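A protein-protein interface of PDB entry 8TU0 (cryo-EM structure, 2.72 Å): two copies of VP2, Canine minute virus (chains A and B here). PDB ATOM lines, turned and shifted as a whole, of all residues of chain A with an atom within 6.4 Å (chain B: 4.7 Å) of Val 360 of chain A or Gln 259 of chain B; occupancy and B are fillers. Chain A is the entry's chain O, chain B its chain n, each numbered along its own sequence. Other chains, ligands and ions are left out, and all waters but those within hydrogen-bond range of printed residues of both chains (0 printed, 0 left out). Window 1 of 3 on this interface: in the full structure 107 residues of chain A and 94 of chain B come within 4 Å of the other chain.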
ATOM      1  N   GLY A 321      31.968  22.791 -26.218  1.00  0.00           N
ATOM      2  CA  GLY A 321      31.715  21.746 -27.171  1.00  0.00           C
ATOM      3  C   GLY A 321      30.591  22.119 -28.093  1.00  0.00           C
ATOM      4  O   GLY A 321      29.730  22.933 -27.755  1.00  0.00           O
ATOM      5  N   PRO A 322      30.572  21.518 -29.280  1.00  0.00           N
ATOM      6  CA  PRO A 322      29.589  21.933 -30.285  1.00  0.00           C
ATOM      7  C   PRO A 322      28.164  21.831 -29.793  1.00  0.00           C
ATOM      8  O   PRO A 322      27.350  22.724 -30.051  1.00  0.00           O
ATOM      9  CB  PRO A 322      29.866  20.970 -31.442  1.00  0.00           C
ATOM     10  CG  PRO A 322      31.282  20.600 -31.274  1.00  0.00           C
ATOM     11  CD  PRO A 322      31.499  20.511 -29.802  1.00  0.00           C
ATOM     12  N   VAL A 323      27.848  20.767 -29.070  1.00  0.00           N
ATOM     13  CA  VAL A 323      26.514  20.523 -28.555  1.00  0.00           C
ATOM     14  C   VAL A 323      26.655  20.217 -27.075  1.00  0.00           C
ATOM     15  O   VAL A 323      27.234  19.189 -26.708  1.00  0.00           O
ATOM     16  CB  VAL A 323      25.823  19.369 -29.286  1.00  0.00           C
ATOM     17  CG1 VAL A 323      24.534  19.006 -28.601  1.00  0.00           C
ATOM     18  CG2 VAL A 323      25.569  19.743 -30.724  1.00  0.00           C
ATOM     19  N   THR A 324      26.133  21.095 -26.228  1.00  0.00           N
ATOM     20  CA  THR A 324      26.063  20.851 -24.797  1.00  0.00           C
ATOM     21  C   THR A 324      24.628  20.531 -24.410  1.00  0.00           C
ATOM     22  O   THR A 324      23.688  21.172 -24.880  1.00  0.00           O
ATOM     23  CB  THR A 324      26.594  22.042 -23.995  1.00  0.00           C
ATOM     24  OG1 THR A 324      26.510  21.756 -22.596  1.00  0.00           O
ATOM     25  CG2 THR A 324      25.832  23.291 -24.295  1.00  0.00           C
ATOM     26  N   VAL A 325      24.465  19.519 -23.568  1.00  0.00           N
ATOM     27  CA  VAL A 325      23.175  18.899 -23.321  1.00  0.00           C
ATOM     28  C   VAL A 325      22.889  18.979 -21.834  1.00  0.00           C
ATOM     29  O   VAL A 325      23.622  18.402 -21.025  1.00  0.00           O
ATOM     30  CB  VAL A 325      23.158  17.441 -23.786  1.00  0.00           C
ATOM     31  CG1 VAL A 325      21.773  16.852 -23.644  1.00  0.00           C
ATOM     32  CG2 VAL A 325      23.671  17.341 -25.183  1.00  0.00           C
ATOM     33  N   THR A 327      20.624  17.735 -19.064  1.00  0.00           N
ATOM     34  CA  THR A 327      19.646  16.726 -18.693  1.00  0.00           C
ATOM     35  C   THR A 327      18.996  17.168 -17.396  1.00  0.00           C
ATOM     36  O   THR A 327      19.645  17.191 -16.347  1.00  0.00           O
ATOM     37  CB  THR A 327      20.297  15.360 -18.525  1.00  0.00           C
ATOM     38  OG1 THR A 327      20.832  14.922 -19.777  1.00  0.00           O
ATOM     39  CG2 THR A 327      19.284  14.356 -18.036  1.00  0.00           C
ATOM     40  N   TYR A 358      26.713  18.784 -20.557  1.00  0.00           N
ATOM     41  CA  TYR A 358      27.794  17.925 -21.003  1.00  0.00           C
ATOM     42  C   TYR A 358      27.895  17.990 -22.514  1.00  0.00           C
ATOM     43  O   TYR A 358      26.941  17.660 -23.218  1.00  0.00           O
ATOM     44  CB  TYR A 358      27.544  16.496 -20.544  1.00  0.00           C
ATOM     45  CG  TYR A 358      27.489  16.370 -19.050  1.00  0.00           C
ATOM     46  CD1 TYR A 358      28.497  16.878 -18.257  1.00  0.00           C
ATOM     47  CD2 TYR A 358      26.393  15.815 -18.434  1.00  0.00           C
ATOM     48  CE1 TYR A 358      28.437  16.782 -16.893  1.00  0.00           C
ATOM     49  CE2 TYR A 358      26.319  15.727 -17.078  1.00  0.00           C
ATOM     50  CZ  TYR A 358      27.342  16.207 -16.307  1.00  0.00           C
ATOM     51  OH  TYR A 358      27.258  16.113 -14.943  1.00  0.00           O
ATOM     52  N   ASP A 359      29.052  18.408 -23.001  1.00  0.00           N
ATOM     53  CA  ASP A 359      29.263  18.595 -24.425  1.00  0.00           C
ATOM     54  C   ASP A 359      29.482  17.268 -25.139  1.00  0.00           C
ATOM     55  O   ASP A 359      29.906  16.276 -24.543  1.00  0.00           O
ATOM     56  CB  ASP A 359      30.456  19.514 -24.638  1.00  0.00           C
ATOM     57  CG  ASP A 359      31.648  19.086 -23.826  1.00  0.00           C
ATOM     58  OD1 ASP A 359      31.479  18.187 -22.979  1.00  0.00           O
ATOM     59  OD2 ASP A 359      32.751  19.638 -24.024  1.00  0.00           O
ATOM     60  N   VAL A 360      29.182  17.251 -26.436  1.00  0.00           N
ATOM     61  CA  VAL A 360      29.479  16.112 -27.299  1.00  0.00           C
ATOM     62  C   VAL A 360      30.347  16.607 -28.447  1.00  0.00           C
ATOM     63  O   VAL A 360      30.014  17.596 -29.110  1.00  0.00           O
ATOM     64  CB  VAL A 360      28.209  15.417 -27.816  1.00  0.00           C
ATOM     65  CG1 VAL A 360      27.418  14.870 -26.671  1.00  0.00           C
ATOM     66  CG2 VAL A 360      27.362  16.350 -28.588  1.00  0.00           C
ATOM     67  N   SER A 361      31.481  15.951 -28.650  1.00  0.00           N
ATOM     68  CA  SER A 361      32.410  16.337 -29.691  1.00  0.00           C
ATOM     69  C   SER A 361      33.143  15.122 -30.221  1.00  0.00           C
ATOM     70  O   SER A 361      33.356  14.167 -29.486  1.00  0.00           O
ATOM     71  CB  SER A 361      33.406  17.360 -29.153  1.00  0.00           C
ATOM     72  OG  SER A 361      34.358  17.724 -30.133  1.00  0.00           O
ATOM     73  N   PRO A 362      33.522  15.139 -31.501  1.00  0.00           N
ATOM     74  CA  PRO A 362      33.077  16.068 -32.537  1.00  0.00           C
ATOM     75  C   PRO A 362      31.724  15.676 -33.072  1.00  0.00           C
ATOM     76  O   PRO A 362      31.390  14.501 -33.071  1.00  0.00           O
ATOM     77  CB  PRO A 362      34.140  15.923 -33.612  1.00  0.00           C
ATOM     78  CG  PRO A 362      34.669  14.572 -33.421  1.00  0.00           C
ATOM     79  CD  PRO A 362      34.639  14.308 -31.966  1.00  0.00           C
ATOM     80  N   VAL A 363      30.936  16.650 -33.497  1.00  0.00           N
ATOM     81  CA  VAL A 363      29.623  16.353 -34.045  1.00  0.00           C
ATOM     82  C   VAL A 363      29.649  16.426 -35.570  1.00  0.00           C
ATOM     83  O   VAL A 363      28.612  16.284 -36.223  1.00  0.00           O
ATOM     84  CB  VAL A 363      28.573  17.293 -33.439  1.00  0.00           C
ATOM     85  CG1 VAL A 363      28.729  18.691 -33.990  1.00  0.00           C
ATOM     86  CG2 VAL A 363      27.182  16.739 -33.625  1.00  0.00           C
ATOM     87  N   PRO B 257      22.996  10.839 -17.181  1.00  0.00           N
ATOM     88  CA  PRO B 257      22.929  11.427 -18.516  1.00  0.00           C
ATOM     89  C   PRO B 257      23.783  10.622 -19.476  1.00  0.00           C
ATOM     90  O   PRO B 257      24.773  10.007 -19.083  1.00  0.00           O
ATOM     91  CB  PRO B 257      23.486  12.833 -18.307  1.00  0.00           C
ATOM     92  CG  PRO B 257      23.203  13.122 -16.891  1.00  0.00           C
ATOM     93  CD  PRO B 257      23.372  11.833 -16.169  1.00  0.00           C
ATOM     94  N   LEU B 258      23.376  10.602 -20.744  1.00  0.00           N
ATOM     95  CA  LEU B 258      24.153   9.867 -21.736  1.00  0.00           C
ATOM     96  C   LEU B 258      25.607  10.288 -21.719  1.00  0.00           C
ATOM     97  O   LEU B 258      26.505   9.466 -21.922  1.00  0.00           O
ATOM     98  CB  LEU B 258      23.574  10.069 -23.132  1.00  0.00           C
ATOM     99  CG  LEU B 258      22.579   9.023 -23.602  1.00  0.00           C
ATOM    100  CD1 LEU B 258      23.223   7.683 -23.507  1.00  0.00           C
ATOM    101  CD2 LEU B 258      21.364   9.056 -22.749  1.00  0.00           C
ATOM    102  N   GLN B 259      25.861  11.564 -21.476  1.00  0.00           N
ATOM    103  CA  GLN B 259      27.184  12.127 -21.635  1.00  0.00           C
ATOM    104  C   GLN B 259      27.947  12.213 -20.329  1.00  0.00           C
ATOM    105  O   GLN B 259      29.111  12.613 -20.333  1.00  0.00           O
ATOM    106  CB  GLN B 259      27.071  13.510 -22.268  1.00  0.00           C
ATOM    107  CG  GLN B 259      26.321  13.484 -23.578  1.00  0.00           C
ATOM    108  CD  GLN B 259      24.833  13.545 -23.370  1.00  0.00           C
ATOM    109  OE1 GLN B 259      24.369  13.701 -22.248  1.00  0.00           O
ATOM    110  NE2 GLN B 259      24.073  13.384 -24.438  1.00  0.00           N
ATOM    111  N   ALA B 260      27.327  11.841 -19.219  1.00  0.00           N
ATOM    112  CA  ALA B 260      27.926  12.001 -17.908  1.00  0.00           C
ATOM    113  C   ALA B 260      28.625  10.755 -17.409  1.00  0.00           C
ATOM    114  O   ALA B 260      29.173  10.775 -16.306  1.00  0.00           O
ATOM    115  CB  ALA B 260      26.866  12.413 -16.894  1.00  0.00           C
ATOM    116  N   ASP B 261      28.632   9.676 -18.178  1.00  0.00           N
ATOM    117  CA  ASP B 261      29.168   8.417 -17.688  1.00  0.00           C
ATOM    118  C   ASP B 261      30.627   8.336 -18.101  1.00  0.00           C
ATOM    119  O   ASP B 261      30.938   8.050 -19.260  1.00  0.00           O
ATOM    120  CB  ASP B 261      28.369   7.243 -18.245  1.00  0.00           C
ATOM    121  CG  ASP B 261      28.702   5.932 -17.559  1.00  0.00           C
ATOM    122  OD1 ASP B 261      29.467   5.954 -16.572  1.00  0.00           O
ATOM    123  OD2 ASP B 261      28.197   4.879 -17.999  1.00  0.00           O
ATOM    124  N   PHE B 262      31.513   8.530 -17.139  1.00  0.00           N
ATOM    125  CA  PHE B 262      32.952   8.475 -17.358  1.00  0.00           C
ATOM    126  C   PHE B 262      33.618   8.485 -15.991  1.00  0.00           C
ATOM    127  O   PHE B 262      32.957   8.585 -14.956  1.00  0.00           O
ATOM    128  CB  PHE B 262      33.449   9.615 -18.248  1.00  0.00           C
ATOM    129  CG  PHE B 262      32.993  10.970 -17.820  1.00  0.00           C
ATOM    130  CD1 PHE B 262      33.640  11.653 -16.821  1.00  0.00           C
ATOM    131  CD2 PHE B 262      31.944  11.584 -18.462  1.00  0.00           C
ATOM    132  CE1 PHE B 262      33.224  12.897 -16.447  1.00  0.00           C
ATOM    133  CE2 PHE B 262      31.532  12.832 -18.094  1.00  0.00           C
ATOM    134  CZ  PHE B 262      32.171  13.486 -17.087  1.00  0.00           C
ATOM    135  N   LYS B 294      34.099  15.671 -19.874  1.00  0.00           N
ATOM    136  CA  LYS B 294      34.660  14.949 -20.991  1.00  0.00           C
ATOM    137  C   LYS B 294      33.681  14.962 -22.150  1.00  0.00           C
ATOM    138  O   LYS B 294      32.467  14.905 -21.942  1.00  0.00           O
ATOM    139  CB  LYS B 294      34.990  13.503 -20.621  1.00  0.00           C
ATOM    140  CG  LYS B 294      36.114  13.388 -19.633  1.00  0.00           C
ATOM    141  CD  LYS B 294      36.358  11.960 -19.231  1.00  0.00           C
ATOM    142  CE  LYS B 294      37.512  11.882 -18.267  1.00  0.00           C
ATOM    143  NZ  LYS B 294      37.742  10.506 -17.775  1.00  0.00           N
ATOM    144  N   SER B 296      31.568  13.575 -25.408  1.00  0.00           N
ATOM    145  CA  SER B 296      30.871  12.320 -25.609  1.00  0.00           C
ATOM    146  C   SER B 296      30.531  12.172 -27.078  1.00  0.00           C
ATOM    147  O   SER B 296      30.477  13.147 -27.825  1.00  0.00           O
ATOM    148  CB  SER B 296      29.600  12.236 -24.768  1.00  0.00           C
ATOM    149  OG  SER B 296      28.940  11.010 -24.996  1.00  0.00           O
ATOM    150  N   TRP B 298      27.658  10.590 -27.890  1.00  0.00           N
ATOM    151  CA  TRP B 298      26.252  10.223 -27.884  1.00  0.00           C
ATOM    152  C   TRP B 298      25.408  11.485 -27.902  1.00  0.00           C
ATOM    153  O   TRP B 298      25.402  12.252 -26.937  1.00  0.00           O
ATOM    154  CB  TRP B 298      25.934   9.331 -26.693  1.00  0.00           C
ATOM    155  CG  TRP B 298      26.741   8.101 -26.758  1.00  0.00           C
ATOM    156  CD1 TRP B 298      27.778   7.765 -25.960  1.00  0.00           C
ATOM    157  CD2 TRP B 298      26.675   7.099 -27.772  1.00  0.00           C
ATOM    158  NE1 TRP B 298      28.320   6.576 -26.363  1.00  0.00           N
ATOM    159  CE2 TRP B 298      27.663   6.152 -27.486  1.00  0.00           C
ATOM    160  CE3 TRP B 298      25.851   6.898 -28.880  1.00  0.00           C
ATOM    161  CZ2 TRP B 298      27.854   5.022 -28.262  1.00  0.00           C
ATOM    162  CZ3 TRP B 298      26.042   5.778 -29.645  1.00  0.00           C
ATOM    163  CH2 TRP B 298      27.034   4.855 -29.336  1.00  0.00           C
ATOM    164  N   MET B 299      24.711  11.695 -29.008  1.00  0.00           N
ATOM    165  CA  MET B 299      23.858  12.847 -29.221  1.00  0.00           C
ATOM    166  C   MET B 299      22.553  12.707 -28.459  1.00  0.00           C
ATOM    167  O   MET B 299      22.168  11.607 -28.062  1.00  0.00           O
ATOM    168  CB  MET B 299      23.562  12.991 -30.704  1.00  0.00           C
ATOM    169  CG  MET B 299      24.729  13.414 -31.540  1.00  0.00           C
ATOM    170  SD  MET B 299      25.185  15.104 -31.168  1.00  0.00           S
ATOM    171  CE  MET B 299      23.736  15.944 -31.800  1.00  0.00           C
ATOM    172  N   PRO B 300      21.849  13.811 -28.242  1.00  0.00           N
ATOM    173  CA  PRO B 300      20.503  13.719 -27.685  1.00  0.00           C
ATOM    174  C   PRO B 300      19.536  13.159 -28.710  1.00  0.00           C
ATOM    175  O   PRO B 300      19.645  13.440 -29.904  1.00  0.00           O
ATOM    176  CB  PRO B 300      20.168  15.170 -27.353  1.00  0.00           C
ATOM    177  CG  PRO B 300      21.441  15.832 -27.252  1.00  0.00           C
ATOM    178  CD  PRO B 300      22.319  15.197 -28.258  1.00  0.00           C
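Val 360 of chain A touches four residues of chain B.
Of chain A, only Tyr 358 (3.5 Å) and Val 360 (3.6 Å) come within 4 Å of Gln 259 of chain B.
Of the printed residues of chain A, Ser 296 of chain B touches Asp 359 (3.3 Å), Val 360 (3.2 Å) and Ser 361 (3.1 Å).
Of the printed residues of chain A, Met 299 of chain B touches Val 360 and Val 363.
Printed residues of chain A within 4 Å of Lys 294 of chain B: Asp 359.
Pro 322 of chain A touches none of the printed residues of chain B.
The nearest printed residue of chain B that does not touch Val 360 of chain A is Pro 300 of chain B (5.2 Å).
Of the 12 printed residues of chain A, 7 touch a printed residue of chain B.
Hydrophobic or aromatic side chains of chain B within 4 Å of the printed part of chain A: Pro 257, Ala 260, Met 299 and Pro 300.
The backbone carbonyl oxygen (O) of Asp 359 of chain A lies within hydrogen-bond range of the backbone NH (N) of Ser 296 of chain B, at 3.3 Å.
N of Ser 361 of chain A is in hydrogen-bond range of O of Ser 296 of chain B.
Among the printed residues, pairs that only touch across the chains: Val 360 of chain A with Ser 296 of chain B (3.2 Å), Val 360 of chain A with Trp 298 of chain B (3.3 Å), Tyr 358 of chain A with Ala 260 of chain B (3.4 Å), Val 325 of chain A with Pro 300 of chain B (3.4 Å), Tyr 358 of chain A with Gln 259 of chain B (3.5 Å), Val 360 of chain A with Gln 259 of chain B (3.6 Å), Val 363 of chain A with Met 299 of chain B (3.6 Å), Asp 359 of chain A with Lys 294 of chain B (3.6 Å), Val 360 of chain A with Met 299 of chain B (3.6 Å) and Thr 327 of chain A with Pro 257 of chain B (3.7 Å).
No position is printed for both chains.
The backbone NH of Val 325 of chain A is in hydrogen-bond range of the backbone carbonyl oxygen of Tyr 358 of chain A.
O of Val 323 of chain A lies within hydrogen-bond range of N of Val 360 of chain A (2.8 Å).
The side-chain hydroxyl (OG) of Ser 296 of chain B lies within hydrogen-bond range of the backbone NH (N) of Trp 298 of chain B.
The side-chain amide nitrogen (NE2) of Gln 259 of chain B sits at hydrogen-bond distance from the backbone carbonyl oxygen (O) of Trp 298 of chain B (3.0 Å).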
